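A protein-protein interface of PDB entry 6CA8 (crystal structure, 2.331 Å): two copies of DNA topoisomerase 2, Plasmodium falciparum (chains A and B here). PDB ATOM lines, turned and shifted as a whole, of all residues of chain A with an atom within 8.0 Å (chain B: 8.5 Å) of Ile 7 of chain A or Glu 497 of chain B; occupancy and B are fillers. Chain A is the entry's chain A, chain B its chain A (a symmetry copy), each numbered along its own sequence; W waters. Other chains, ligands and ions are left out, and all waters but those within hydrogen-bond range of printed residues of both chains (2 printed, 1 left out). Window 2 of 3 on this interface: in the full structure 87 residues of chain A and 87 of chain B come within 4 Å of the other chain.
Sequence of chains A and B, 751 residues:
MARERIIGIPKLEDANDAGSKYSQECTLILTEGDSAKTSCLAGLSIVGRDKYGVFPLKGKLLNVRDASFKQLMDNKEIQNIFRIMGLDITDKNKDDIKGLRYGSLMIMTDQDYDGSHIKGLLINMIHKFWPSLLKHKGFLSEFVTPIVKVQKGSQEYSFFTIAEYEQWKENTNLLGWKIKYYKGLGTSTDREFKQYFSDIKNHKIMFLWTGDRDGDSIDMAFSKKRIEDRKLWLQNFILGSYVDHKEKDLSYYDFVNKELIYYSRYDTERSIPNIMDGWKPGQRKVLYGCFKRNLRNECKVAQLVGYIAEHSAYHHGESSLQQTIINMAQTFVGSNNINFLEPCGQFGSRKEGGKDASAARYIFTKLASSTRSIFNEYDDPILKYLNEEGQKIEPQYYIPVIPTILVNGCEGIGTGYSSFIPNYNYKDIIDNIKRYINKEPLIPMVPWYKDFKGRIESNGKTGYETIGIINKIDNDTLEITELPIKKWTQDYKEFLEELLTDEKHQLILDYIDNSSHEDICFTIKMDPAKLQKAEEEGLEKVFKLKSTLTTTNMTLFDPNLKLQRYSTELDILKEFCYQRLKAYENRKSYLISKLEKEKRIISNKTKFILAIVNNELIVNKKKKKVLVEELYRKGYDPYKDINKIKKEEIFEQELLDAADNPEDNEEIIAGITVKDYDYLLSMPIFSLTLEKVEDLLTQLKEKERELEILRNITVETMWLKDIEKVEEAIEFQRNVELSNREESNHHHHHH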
ATOM      1  N   GLU A   4     -13.961  10.271 -21.155  1.00  0.00           N
ATOM      2  CA  GLU A   4     -14.615   9.458 -22.181  1.00  0.00           C
ATOM      3  C   GLU A   4     -16.129   9.651 -22.062  1.00  0.00           C
ATOM      4  O   GLU A   4     -16.652   9.777 -20.956  1.00  0.00           O
ATOM      5  CB  GLU A   4     -14.239   7.987 -22.099  1.00  0.00           C
ATOM      6  CG  GLU A   4     -13.438   7.594 -23.324  1.00  0.00           C
ATOM      7  CD  GLU A   4     -14.309   7.359 -24.537  1.00  0.00           C
ATOM      8  OE1 GLU A   4     -15.419   6.805 -24.388  1.00  0.00           O
ATOM      9  OE2 GLU A   4     -13.894   7.793 -25.634  1.00  0.00           O
ATOM     10  N   ARG A   5     -16.824   9.715 -23.196  1.00  0.00           N
ATOM     11  CA  ARG A   5     -18.285   9.710 -23.165  1.00  0.00           C
ATOM     12  C   ARG A   5     -18.940   9.131 -24.420  1.00  0.00           C
ATOM     13  O   ARG A   5     -18.343   9.106 -25.500  1.00  0.00           O
ATOM     14  CB  ARG A   5     -18.738  11.181 -22.975  1.00  0.00           C
ATOM     15  CG  ARG A   5     -20.118  11.574 -23.526  1.00  0.00           C
ATOM     16  CD  ARG A   5     -20.388  13.107 -23.553  1.00  0.00           C
ATOM     17  NE  ARG A   5     -20.745  13.596 -24.903  1.00  0.00           N
ATOM     18  CZ  ARG A   5     -20.090  14.529 -25.595  1.00  0.00           C
ATOM     19  NH1 ARG A   5     -19.022  15.138 -25.096  1.00  0.00           N
ATOM     20  NH2 ARG A   5     -20.533  14.864 -26.799  1.00  0.00           N
ATOM     21  N   ILE A   6     -20.169   8.648 -24.252  1.00  0.00           N
ATOM     22  CA  ILE A   6     -20.900   7.949 -25.297  1.00  0.00           C
ATOM     23  C   ILE A   6     -21.918   8.875 -25.927  1.00  0.00           C
ATOM     24  O   ILE A   6     -22.661   9.569 -25.229  1.00  0.00           O
ATOM     25  CB  ILE A   6     -21.622   6.714 -24.750  1.00  0.00           C
ATOM     26  CG1 ILE A   6     -20.702   5.907 -23.832  1.00  0.00           C
ATOM     27  CG2 ILE A   6     -22.066   5.841 -25.887  1.00  0.00           C
ATOM     28  CD1 ILE A   6     -19.550   5.240 -24.552  1.00  0.00           C
ATOM     29  N   ILE A   7     -21.949   8.881 -27.254  1.00  0.00           N
ATOM     30  CA  ILE A   7     -22.758   9.840 -27.990  1.00  0.00           C
ATOM     31  C   ILE A   7     -24.135   9.323 -28.414  1.00  0.00           C
ATOM     32  O   ILE A   7     -25.138   9.985 -28.178  1.00  0.00           O
ATOM     33  CB  ILE A   7     -21.989  10.328 -29.236  1.00  0.00           C
ATOM     34  CG1 ILE A   7     -20.916  11.338 -28.820  1.00  0.00           C
ATOM     35  CG2 ILE A   7     -22.937  10.919 -30.275  1.00  0.00           C
ATOM     36  CD1 ILE A   7     -19.549  11.058 -29.406  1.00  0.00           C
ATOM     37  N   GLY A   8     -24.190   8.151 -29.038  1.00  0.00           N
ATOM     38  CA  GLY A   8     -25.348   7.789 -29.841  1.00  0.00           C
ATOM     39  C   GLY A   8     -26.443   6.954 -29.194  1.00  0.00           C
ATOM     40  O   GLY A   8     -27.275   6.382 -29.899  1.00  0.00           O
ATOM     41  N   ILE A   9     -26.450   6.871 -27.866  1.00  0.00           N
ATOM     42  CA  ILE A   9     -27.298   5.895 -27.179  1.00  0.00           C
ATOM     43  C   ILE A   9     -28.140   6.491 -26.052  1.00  0.00           C
ATOM     44  O   ILE A   9     -27.735   6.474 -24.888  1.00  0.00           O
ATOM     45  CB  ILE A   9     -26.470   4.728 -26.600  1.00  0.00           C
ATOM     46  CG1 ILE A   9     -25.542   4.146 -27.665  1.00  0.00           C
ATOM     47  CG2 ILE A   9     -27.382   3.630 -26.092  1.00  0.00           C
ATOM     48  CD1 ILE A   9     -24.315   3.487 -27.108  1.00  0.00           C
ATOM     49  N   PRO A  10     -29.298   7.068 -26.407  1.00  0.00           N
ATOM     50  CA  PRO A  10     -30.107   7.838 -25.455  1.00  0.00           C
ATOM     51  C   PRO A  10     -30.566   6.995 -24.265  1.00  0.00           C
ATOM     52  O   PRO A  10     -30.696   7.510 -23.155  1.00  0.00           O
ATOM     53  CB  PRO A  10     -31.319   8.288 -26.287  1.00  0.00           C
ATOM     54  CG  PRO A  10     -31.242   7.532 -27.574  1.00  0.00           C
ATOM     55  CD  PRO A  10     -29.814   7.172 -27.782  1.00  0.00           C
ATOM     56  N   LYS A  11     -30.818   5.712 -24.505  1.00  0.00           N
ATOM     57  CA  LYS A  11     -31.310   4.820 -23.459  1.00  0.00           C
ATOM     58  C   LYS A  11     -30.247   4.448 -22.419  1.00  0.00           C
ATOM     59  O   LYS A  11     -30.581   3.970 -21.332  1.00  0.00           O
ATOM     60  CB  LYS A  11     -31.899   3.549 -24.087  1.00  0.00           C
ATOM     61  CG  LYS A  11     -33.201   3.789 -24.842  1.00  0.00           C
ATOM     62  CD  LYS A  11     -33.997   2.507 -25.021  1.00  0.00           C
ATOM     63  CE  LYS A  11     -35.430   2.804 -25.447  1.00  0.00           C
ATOM     64  NZ  LYS A  11     -36.118   3.743 -24.511  1.00  0.00           N
ATOM     65  N   LEU A  12     -28.976   4.647 -22.754  1.00  0.00           N
ATOM     66  CA  LEU A  12     -27.885   4.358 -21.822  1.00  0.00           C
ATOM     67  C   LEU A  12     -27.885   5.291 -20.609  1.00  0.00           C
ATOM     68  O   LEU A  12     -27.921   6.512 -20.755  1.00  0.00           O
ATOM     69  CB  LEU A  12     -26.534   4.438 -22.547  1.00  0.00           C
ATOM     70  CG  LEU A  12     -25.239   4.375 -21.724  1.00  0.00           C
ATOM     71  CD1 LEU A  12     -25.119   3.046 -20.999  1.00  0.00           C
ATOM     72  CD2 LEU A  12     -24.014   4.614 -22.607  1.00  0.00           C
ATOM     73  N   ASP A  14     -25.106   5.789 -18.492  1.00  0.00           N
ATOM     74  CA  ASP A  14     -23.679   5.567 -18.290  1.00  0.00           C
ATOM     75  C   ASP A  14     -23.221   5.920 -16.877  1.00  0.00           C
ATOM     76  O   ASP A  14     -23.622   6.945 -16.323  1.00  0.00           O
ATOM     77  CB  ASP A  14     -22.884   6.390 -19.310  1.00  0.00           C
ATOM     78  CG  ASP A  14     -21.575   5.732 -19.706  1.00  0.00           C
ATOM     79  OD1 ASP A  14     -21.535   4.485 -19.776  1.00  0.00           O
ATOM     80  OD2 ASP A  14     -20.587   6.456 -19.954  1.00  0.00           O
ATOM     81  N   ASN A  80     -24.513  -1.330 -30.081  1.00  0.00           N
ATOM     82  CA  ASN A  80     -24.558  -0.427 -28.944  1.00  0.00           C
ATOM     83  C   ASN A  80     -23.939  -1.036 -27.703  1.00  0.00           C
ATOM     84  O   ASN A  80     -23.201  -0.364 -26.993  1.00  0.00           O
ATOM     85  CB  ASN A  80     -26.000  -0.027 -28.635  1.00  0.00           C
ATOM     86  CG  ASN A  80     -26.479   1.131 -29.481  1.00  0.00           C
ATOM     87  OD1 ASN A  80     -25.688   1.971 -29.902  1.00  0.00           O
ATOM     88  ND2 ASN A  80     -27.786   1.199 -29.706  1.00  0.00           N
ATOM     89  N   ARG A  83     -20.247  -0.830 -28.082  1.00  0.00           N
ATOM     90  CA  ARG A  83     -19.744   0.518 -27.819  1.00  0.00           C
ATOM     91  C   ARG A  83     -19.755   0.898 -26.338  1.00  0.00           C
ATOM     92  O   ARG A  83     -18.808   1.508 -25.840  1.00  0.00           O
ATOM     93  CB  ARG A  83     -20.538   1.546 -28.624  1.00  0.00           C
ATOM     94  CG  ARG A  83     -20.397   1.375 -30.131  1.00  0.00           C
ATOM     95  CD  ARG A  83     -21.218   2.405 -30.881  1.00  0.00           C
ATOM     96  NE  ARG A  83     -21.063   3.740 -30.313  1.00  0.00           N
ATOM     97  CZ  ARG A  83     -22.042   4.635 -30.237  1.00  0.00           C
ATOM     98  NH1 ARG A  83     -23.251   4.335 -30.689  1.00  0.00           N
ATOM     99  NH2 ARG A  83     -21.812   5.828 -29.709  1.00  0.00           N
ATOM    100  N   GLN B 490     -36.386  11.372 -20.099  1.00  0.00           N
ATOM    101  CA  GLN B 490     -35.709  10.840 -21.271  1.00  0.00           C
ATOM    102  C   GLN B 490     -35.805  11.749 -22.506  1.00  0.00           C
ATOM    103  O   GLN B 490     -34.806  11.942 -23.219  1.00  0.00           O
ATOM    104  CB  GLN B 490     -36.291   9.464 -21.608  1.00  0.00           C
ATOM    105  CG  GLN B 490     -35.699   8.835 -22.848  1.00  0.00           C
ATOM    106  CD  GLN B 490     -34.297   8.332 -22.596  1.00  0.00           C
ATOM    107  OE1 GLN B 490     -33.977   7.886 -21.494  1.00  0.00           O
ATOM    108  NE2 GLN B 490     -33.444   8.415 -23.608  1.00  0.00           N
ATOM    109  N   ASP B 491     -36.970  12.352 -22.726  1.00  0.00           N
ATOM    110  CA  ASP B 491     -37.117  13.311 -23.822  1.00  0.00           C
ATOM    111  C   ASP B 491     -36.213  14.525 -23.648  1.00  0.00           C
ATOM    112  O   ASP B 491     -35.556  14.984 -24.593  1.00  0.00           O
ATOM    113  CB  ASP B 491     -38.572  13.781 -23.928  1.00  0.00           C
ATOM    114  CG  ASP B 491     -39.534  12.652 -24.236  1.00  0.00           C
ATOM    115  OD1 ASP B 491     -39.138  11.707 -24.946  1.00  0.00           O
ATOM    116  OD2 ASP B 491     -40.687  12.706 -23.755  1.00  0.00           O
ATOM    117  N   TYR B 492     -36.145  15.015 -22.417  1.00  0.00           N
ATOM    118  CA  TYR B 492     -35.292  16.148 -22.109  1.00  0.00           C
ATOM    119  C   TYR B 492     -33.816  15.822 -22.294  1.00  0.00           C
ATOM    120  O   TYR B 492     -33.045  16.649 -22.797  1.00  0.00           O
ATOM    121  CB  TYR B 492     -35.537  16.665 -20.697  1.00  0.00           C
ATOM    122  CG  TYR B 492     -34.960  18.047 -20.543  1.00  0.00           C
ATOM    123  CD1 TYR B 492     -35.688  19.161 -20.930  1.00  0.00           C
ATOM    124  CD2 TYR B 492     -33.677  18.236 -20.055  1.00  0.00           C
ATOM    125  CE1 TYR B 492     -35.169  20.429 -20.804  1.00  0.00           C
ATOM    126  CE2 TYR B 492     -33.142  19.503 -19.934  1.00  0.00           C
ATOM    127  CZ  TYR B 492     -33.897  20.596 -20.307  1.00  0.00           C
ATOM    128  OH  TYR B 492     -33.367  21.859 -20.206  1.00  0.00           O
ATOM    129  N   LYS B 493     -33.425  14.621 -21.878  1.00  0.00           N
ATOM    130  CA  LYS B 493     -32.051  14.182 -22.060  1.00  0.00           C
ATOM    131  C   LYS B 493     -31.697  14.138 -23.539  1.00  0.00           C
ATOM    132  O   LYS B 493     -30.593  14.537 -23.940  1.00  0.00           O
ATOM    133  CB  LYS B 493     -31.861  12.792 -21.455  1.00  0.00           C
ATOM    134  CG  LYS B 493     -30.448  12.256 -21.554  1.00  0.00           C
ATOM    135  CD  LYS B 493     -30.487  10.802 -22.003  1.00  0.00           C
ATOM    136  CE  LYS B 493     -29.150  10.113 -21.832  1.00  0.00           C
ATOM    137  NZ  LYS B 493     -29.196   9.103 -20.741  1.00  0.00           N
ATOM    138  N   GLU B 494     -32.637  13.664 -24.352  1.00  0.00           N
ATOM    139  CA  GLU B 494     -32.405  13.656 -25.790  1.00  0.00           C
ATOM    140  C   GLU B 494     -32.244  15.088 -26.309  1.00  0.00           C
ATOM    141  O   GLU B 494     -31.426  15.346 -27.189  1.00  0.00           O
ATOM    142  CB  GLU B 494     -33.520  12.912 -26.529  1.00  0.00           C
ATOM    143  CG  GLU B 494     -33.416  11.390 -26.390  1.00  0.00           C
ATOM    144  CD  GLU B 494     -34.516  10.647 -27.123  1.00  0.00           C
ATOM    145  OE1 GLU B 494     -35.103   9.714 -26.535  1.00  0.00           O
ATOM    146  OE2 GLU B 494     -34.785  10.987 -28.294  1.00  0.00           O
ATOM    147  N   PHE B 495     -33.019  16.018 -25.756  1.00  0.00           N
ATOM    148  CA  PHE B 495     -32.893  17.425 -26.140  1.00  0.00           C
ATOM    149  C   PHE B 495     -31.519  18.027 -25.794  1.00  0.00           C
ATOM    150  O   PHE B 495     -30.925  18.751 -26.612  1.00  0.00           O
ATOM    151  CB  PHE B 495     -34.031  18.237 -25.503  1.00  0.00           C
ATOM    152  CG  PHE B 495     -33.737  19.703 -25.359  1.00  0.00           C
ATOM    153  CD1 PHE B 495     -33.911  20.571 -26.427  1.00  0.00           C
ATOM    154  CD2 PHE B 495     -33.352  20.223 -24.134  1.00  0.00           C
ATOM    155  CE1 PHE B 495     -33.651  21.926 -26.287  1.00  0.00           C
ATOM    156  CE2 PHE B 495     -33.099  21.574 -23.986  1.00  0.00           C
ATOM    157  CZ  PHE B 495     -33.250  22.426 -25.062  1.00  0.00           C
ATOM    158  N   LEU B 496     -30.993  17.708 -24.612  1.00  0.00           N
ATOM    159  CA  LEU B 496     -29.633  18.141 -24.262  1.00  0.00           C
ATOM    160  C   LEU B 496     -28.579  17.537 -25.184  1.00  0.00           C
ATOM    161  O   LEU B 496     -27.626  18.218 -25.637  1.00  0.00           O
ATOM    162  CB  LEU B 496     -29.309  17.770 -22.808  1.00  0.00           C
ATOM    163  CG  LEU B 496     -30.032  18.510 -21.675  1.00  0.00           C
ATOM    164  CD1 LEU B 496     -29.534  18.020 -20.323  1.00  0.00           C
ATOM    165  CD2 LEU B 496     -29.850  20.019 -21.803  1.00  0.00           C
ATOM    166  N   GLU B 497     -28.787  16.272 -25.537  1.00  0.00           N
ATOM    167  CA  GLU B 497     -27.863  15.640 -26.475  1.00  0.00           C
ATOM    168  C   GLU B 497     -27.901  16.330 -27.826  1.00  0.00           C
ATOM    169  O   GLU B 497     -26.861  16.515 -28.454  1.00  0.00           O
ATOM    170  CB  GLU B 497     -28.180  14.181 -26.649  1.00  0.00           C
ATOM    171  CG  GLU B 497     -27.000  13.366 -27.158  1.00  0.00           C
ATOM    172  CD  GLU B 497     -26.888  12.025 -26.474  1.00  0.00           C
ATOM    173  OE1 GLU B 497     -26.641  12.008 -25.253  1.00  0.00           O
ATOM    174  OE2 GLU B 497     -27.049  10.989 -27.155  1.00  0.00           O
ATOM    175  N   GLU B 498     -29.080  16.718 -28.304  1.00  0.00           N
ATOM    176  CA  GLU B 498     -29.153  17.432 -29.573  1.00  0.00           C
ATOM    177  C   GLU B 498     -28.507  18.818 -29.438  1.00  0.00           C
ATOM    178  O   GLU B 498     -27.988  19.317 -30.417  1.00  0.00           O
ATOM    179  CB  GLU B 498     -30.588  17.448 -30.132  1.00  0.00           C
ATOM    180  CG  GLU B 498     -31.214  18.773 -30.518  1.00  0.00           C
ATOM    181  CD  GLU B 498     -32.691  18.571 -30.743  1.00  0.00           C
ATOM    182  OE1 GLU B 498     -33.123  17.921 -31.753  1.00  0.00           O
ATOM    183  OE2 GLU B 498     -33.401  18.991 -29.840  1.00  0.00           O
ATOM    184  N   LEU B 499     -28.524  19.405 -28.235  1.00  0.00           N
ATOM    185  CA  LEU B 499     -27.792  20.659 -28.045  1.00  0.00           C
ATOM    186  C   LEU B 499     -26.288  20.460 -28.216  1.00  0.00           C
ATOM    187  O   LEU B 499     -25.585  21.372 -28.670  1.00  0.00           O
ATOM    188  CB  LEU B 499     -28.071  21.284 -26.680  1.00  0.00           C
ATOM    189  CG  LEU B 499     -29.465  21.881 -26.492  1.00  0.00           C
ATOM    190  CD1 LEU B 499     -29.622  22.400 -25.074  1.00  0.00           C
ATOM    191  CD2 LEU B 499     -29.679  22.990 -27.515  1.00  0.00           C
ATOM    192  N   LEU B 500     -25.793  19.276 -27.868  1.00  0.00           N
ATOM    193  CA  LEU B 500     -24.365  18.986 -28.027  1.00  0.00           C
ATOM    194  C   LEU B 500     -23.857  19.044 -29.487  1.00  0.00           C
ATOM    195  O   LEU B 500     -22.730  19.467 -29.739  1.00  0.00           O
ATOM    196  CB  LEU B 500     -24.060  17.595 -27.446  1.00  0.00           C
ATOM    197  CG  LEU B 500     -22.951  17.363 -26.420  1.00  0.00           C
ATOM    198  CD1 LEU B 500     -22.780  18.564 -25.540  1.00  0.00           C
ATOM    199  CD2 LEU B 500     -23.280  16.166 -25.549  1.00  0.00           C
ATOM    200  N   THR B 501     -24.702  18.622 -30.427  1.00  0.00           N
ATOM    201  CA  THR B 501     -24.406  18.610 -31.868  1.00  0.00           C
ATOM    202  C   THR B 501     -24.498  19.970 -32.580  1.00  0.00           C
ATOM    203  O   THR B 501     -25.275  20.834 -32.167  1.00  0.00           O
ATOM    204  CB  THR B 501     -25.341  17.636 -32.601  1.00  0.00           C
ATOM    205  OG1 THR B 501     -26.551  18.310 -32.957  1.00  0.00           O
ATOM    206  CG2 THR B 501     -25.670  16.432 -31.720  1.00  0.00           C
ATOM    207  N   ASP B 502     -23.716  20.152 -33.648  1.00  0.00           N
ATOM    208  CA  ASP B 502     -23.579  21.457 -34.304  1.00  0.00           C
ATOM    209  C   ASP B 502     -24.854  21.941 -34.960  1.00  0.00           C
ATOM    210  O   ASP B 502     -24.969  23.122 -35.275  1.00  0.00           O
ATOM    211  CB  ASP B 502     -22.471  21.453 -35.354  1.00  0.00           C
ATOM    212  CG  ASP B 502     -21.660  22.737 -35.340  1.00  0.00           C
ATOM    213  OD1 ASP B 502     -20.590  22.758 -34.689  1.00  0.00           O
ATOM    214  OD2 ASP B 502     -22.085  23.725 -35.969  1.00  0.00           O
ATOM    215  N   GLU B 503     -25.802  21.041 -35.196  1.00  0.00           N
ATOM    216  CA  GLU B 503     -27.042  21.450 -35.842  1.00  0.00           C
ATOM    217  C   GLU B 503     -27.756  22.405 -34.894  1.00  0.00           C
ATOM    218  O   GLU B 503     -28.651  23.146 -35.296  1.00  0.00           O
ATOM    219  CB  GLU B 503     -27.921  20.242 -36.176  1.00  0.00           C
ATOM    220  N   LYS B 504     -27.331  22.391 -33.633  1.00  0.00           N
ATOM    221  CA  LYS B 504     -27.841  23.321 -32.638  1.00  0.00           C
ATOM    222  C   LYS B 504     -26.714  24.235 -32.148  1.00  0.00           C
ATOM    223  O   LYS B 504     -26.747  24.733 -31.022  1.00  0.00           O
ATOM    224  CB  LYS B 504     -28.460  22.568 -31.459  1.00  0.00           C
ATOM    225  N   GLN B 506     -23.645  23.873 -31.094  1.00  0.00           N
ATOM    226  CA  GLN B 506     -22.753  23.518 -29.988  1.00  0.00           C
ATOM    227  C   GLN B 506     -23.055  24.362 -28.744  1.00  0.00           C
ATOM    228  O   GLN B 506     -22.150  24.934 -28.131  1.00  0.00           O
ATOM    229  CB  GLN B 506     -21.284  23.675 -30.413  1.00  0.00           C
ATOM    230  CG  GLN B 506     -20.264  23.068 -29.445  1.00  0.00           C
ATOM    231  CD  GLN B 506     -20.091  21.574 -29.627  1.00  0.00           C
ATOM    232  OE1 GLN B 506     -19.524  21.122 -30.621  1.00  0.00           O
ATOM    233  NE2 GLN B 506     -20.582  20.799 -28.666  1.00  0.00           N
ATOM    234  N   LEU B 507     -24.334  24.480 -28.398  1.00  0.00           N
ATOM    235  CA  LEU B 507     -24.729  25.368 -27.308  1.00  0.00           C
ATOM    236  C   LEU B 507     -24.059  24.944 -26.002  1.00  0.00           C
ATOM    237  O   LEU B 507     -23.657  25.787 -25.202  1.00  0.00           O
ATOM    238  CB  LEU B 507     -26.251  25.379 -27.143  1.00  0.00           C
ATOM    239  CG  LEU B 507     -26.816  26.218 -25.994  1.00  0.00           C
ATOM    240  CD1 LEU B 507     -26.446  27.684 -26.173  1.00  0.00           C
ATOM    241  CD2 LEU B 507     -28.325  26.047 -25.878  1.00  0.00           C
ATOM    242  N   ILE B 508     -23.933  23.639 -25.790  1.00  0.00           N
ATOM    243  CA  ILE B 508     -23.308  23.139 -24.574  1.00  0.00           C
ATOM    244  C   ILE B 508     -22.110  22.251 -24.922  1.00  0.00           C
ATOM    245  O   ILE B 508     -22.116  21.543 -25.930  1.00  0.00           O
ATOM    246  CB  ILE B 508     -24.328  22.396 -23.678  1.00  0.00           C
ATOM    247  CG1 ILE B 508     -24.814  21.110 -24.338  1.00  0.00           C
ATOM    248  CG2 ILE B 508     -25.526  23.284 -23.394  1.00  0.00           C
ATOM    249  CD1 ILE B 508     -25.296  20.067 -23.351  1.00  0.00           C
ATOM    250  N   ASP B 510     -20.882  19.855 -22.575  1.00  0.00           N
ATOM    251  CA  ASP B 510     -21.046  18.521 -21.996  1.00  0.00           C
ATOM    252  C   ASP B 510     -22.167  18.470 -20.971  1.00  0.00           C
ATOM    253  O   ASP B 510     -22.617  19.493 -20.503  1.00  0.00           O
ATOM    254  CB  ASP B 510     -19.724  18.079 -21.350  1.00  0.00           C
ATOM    255  CG  ASP B 510     -19.795  16.690 -20.749  1.00  0.00           C
ATOM    256  OD1 ASP B 510     -20.268  15.765 -21.442  1.00  0.00           O
ATOM    257  OD2 ASP B 510     -19.372  16.522 -19.585  1.00  0.00           O
ATOM    258  N   TYR B 511     -22.698  17.283 -20.706  1.00  0.00           N
ATOM    259  CA  TYR B 511     -23.672  17.141 -19.633  1.00  0.00           C
ATOM    260  C   TYR B 511     -23.546  15.777 -18.957  1.00  0.00           C
ATOM    261  O   TYR B 511     -23.181  14.788 -19.591  1.00  0.00           O
ATOM    262  CB  TYR B 511     -25.097  17.353 -20.152  1.00  0.00           C
ATOM    263  CG  TYR B 511     -25.673  16.151 -20.852  1.00  0.00           C
ATOM    264  CD1 TYR B 511     -25.485  15.963 -22.213  1.00  0.00           C
ATOM    265  CD2 TYR B 511     -26.404  15.201 -20.152  1.00  0.00           C
ATOM    266  CE1 TYR B 511     -26.012  14.867 -22.857  1.00  0.00           C
ATOM    267  CE2 TYR B 511     -26.925  14.097 -20.784  1.00  0.00           C
ATOM    268  CZ  TYR B 511     -26.730  13.937 -22.139  1.00  0.00           C
ATOM    269  OH  TYR B 511     -27.245  12.836 -22.777  1.00  0.00           O
ATOM    270  N   ASP B 513     -26.079  13.239 -16.700  1.00  0.00           N
ATOM    271  CA  ASP B 513     -27.433  13.028 -16.215  1.00  0.00           C
ATOM    272  C   ASP B 513     -27.425  11.967 -15.120  1.00  0.00           C
ATOM    273  O   ASP B 513     -27.185  10.790 -15.386  1.00  0.00           O
ATOM    274  CB  ASP B 513     -28.358  12.619 -17.364  1.00  0.00           C
ATOM    275  CG  ASP B 513     -29.696  12.075 -16.884  1.00  0.00           C
ATOM    276  OD1 ASP B 513     -30.140  12.443 -15.777  1.00  0.00           O
ATOM    277  OD2 ASP B 513     -30.306  11.269 -17.618  1.00  0.00           O
ATOM    278  N   PHE B 522     -29.503  17.221 -13.909  1.00  0.00           N
ATOM    279  CA  PHE B 522     -28.623  17.385 -15.060  1.00  0.00           C
ATOM    280  C   PHE B 522     -27.539  18.404 -14.738  1.00  0.00           C
ATOM    281  O   PHE B 522     -27.831  19.490 -14.260  1.00  0.00           O
ATOM    282  CB  PHE B 522     -29.403  17.851 -16.295  1.00  0.00           C
ATOM    283  CG  PHE B 522     -30.390  16.846 -16.820  1.00  0.00           C
ATOM    284  CD1 PHE B 522     -29.982  15.833 -17.668  1.00  0.00           C
ATOM    285  CD2 PHE B 522     -31.735  16.938 -16.491  1.00  0.00           C
ATOM    286  CE1 PHE B 522     -30.891  14.917 -18.167  1.00  0.00           C
ATOM    287  CE2 PHE B 522     -32.649  16.023 -16.985  1.00  0.00           C
ATOM    288  CZ  PHE B 522     -32.225  15.010 -17.822  1.00  0.00           C
HETATM  289  O   HOH W   1     -26.738  11.848 -29.962  1.00  0.00           O
HETATM  290  O   HOH W   2     -26.231   7.784 -15.668  1.00  0.00           O
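The guanidinium group of Arg 5 of chain A lies within salt-bridge range of the side-chain carboxylate of Asp 510 of chain B. The backbone carbonyl oxygen of Leu 12 of chain A sits at hydrogen-bond distance from the side-chain amino group of Lys 493 of chain B (2.9 Å). The backbone carbonyl oxygen (O) of Pro 10 of chain A sits at hydrogen-bond distance from the side-chain amide nitrogen (NE2) of Gln 490 of chain B, 2.9 Å away. The backbone carbonyl oxygen (O) of Pro 10 of chain A sits at hydrogen-bond distance from the side-chain amino group (NZ) of Lys 493 of chain B (3.3 Å). The side-chain carboxylate (OE2) of Glu 497 of chain B sits close to the backbone carbonyl oxygen (O) of Ile 7 of chain A.
Arg 5 of chain A touches Leu 500 of chain B (NH2 to CD2, 3.3 Å). CG of Glu 494 of chain B touches CB of Pro 10 of chain A, at 3.7 Å. Lys 11 of chain A touches Gln 490 of chain B.
Of the 12 printed residues of chain A, 5 touch a printed residue of chain B. Hydrophobic or aromatic side chains of chain A that line the printed part of chain B: Pro 10. Of the 22 printed residues of chain B, 6 touch a printed residue of chain A. Printed residues of chain B that touch a printed residue of chain A: Gln 490, Lys 493, Glu 494, Glu 497, Leu 500 and Asp 510. Hydrophobic or aromatic side chains of chain B within 4 Å of the printed part of chain A: Leu 500. Among the printed residues, Asp or Glu carboxylates within 4 Å of a Lys or Arg side-chain nitrogen of the other chain: Arg 5 of chain A with Asp 510 of chain B.
Water W2 bridges O of Asp 14 of chain A and O of Asp 513 of chain B. Water W1 lies within hydrogen-bond range of OE2 of Glu 497 of chain B and O of Ile 7 of chain A.
No position is printed for both chains.
Of chain A, only Ile 7 comes within 4 Å of Glu 497 of chain B. Printed residues of chain B within 4 Å of Leu 12 of chain A: Lys 493 (2.9 Å). Printed residues of chain B within 4 Å of Lys 11 of chain A: Gln 490 (3.9 Å). Printed residues of chain A within 4 Å of Gln 490 of chain B: Pro 10 and Lys 11. Printed residues of chain A within 4 Å of Asp 510 of chain B: Arg 5 (3.4 Å). Of the printed residues of chain A, Glu 494 of chain B touches Pro 10 (3.7 Å).
The side-chain hydroxyl of Tyr 511 of chain B sits at hydrogen-bond distance from the side-chain carboxylate of Glu 497 of chain B, 2.7 Å away. The side-chain amino group (NZ) of Lys 493 of chain B lies within salt-bridge range of the side-chain carboxylate (OD2) of Asp 513 of chain B, at 3.96 Å. The side-chain amide nitrogen of Gln 506 of chain B lies within hydrogen-bond range of the backbone carbonyl oxygen of Leu 500 of chain B.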
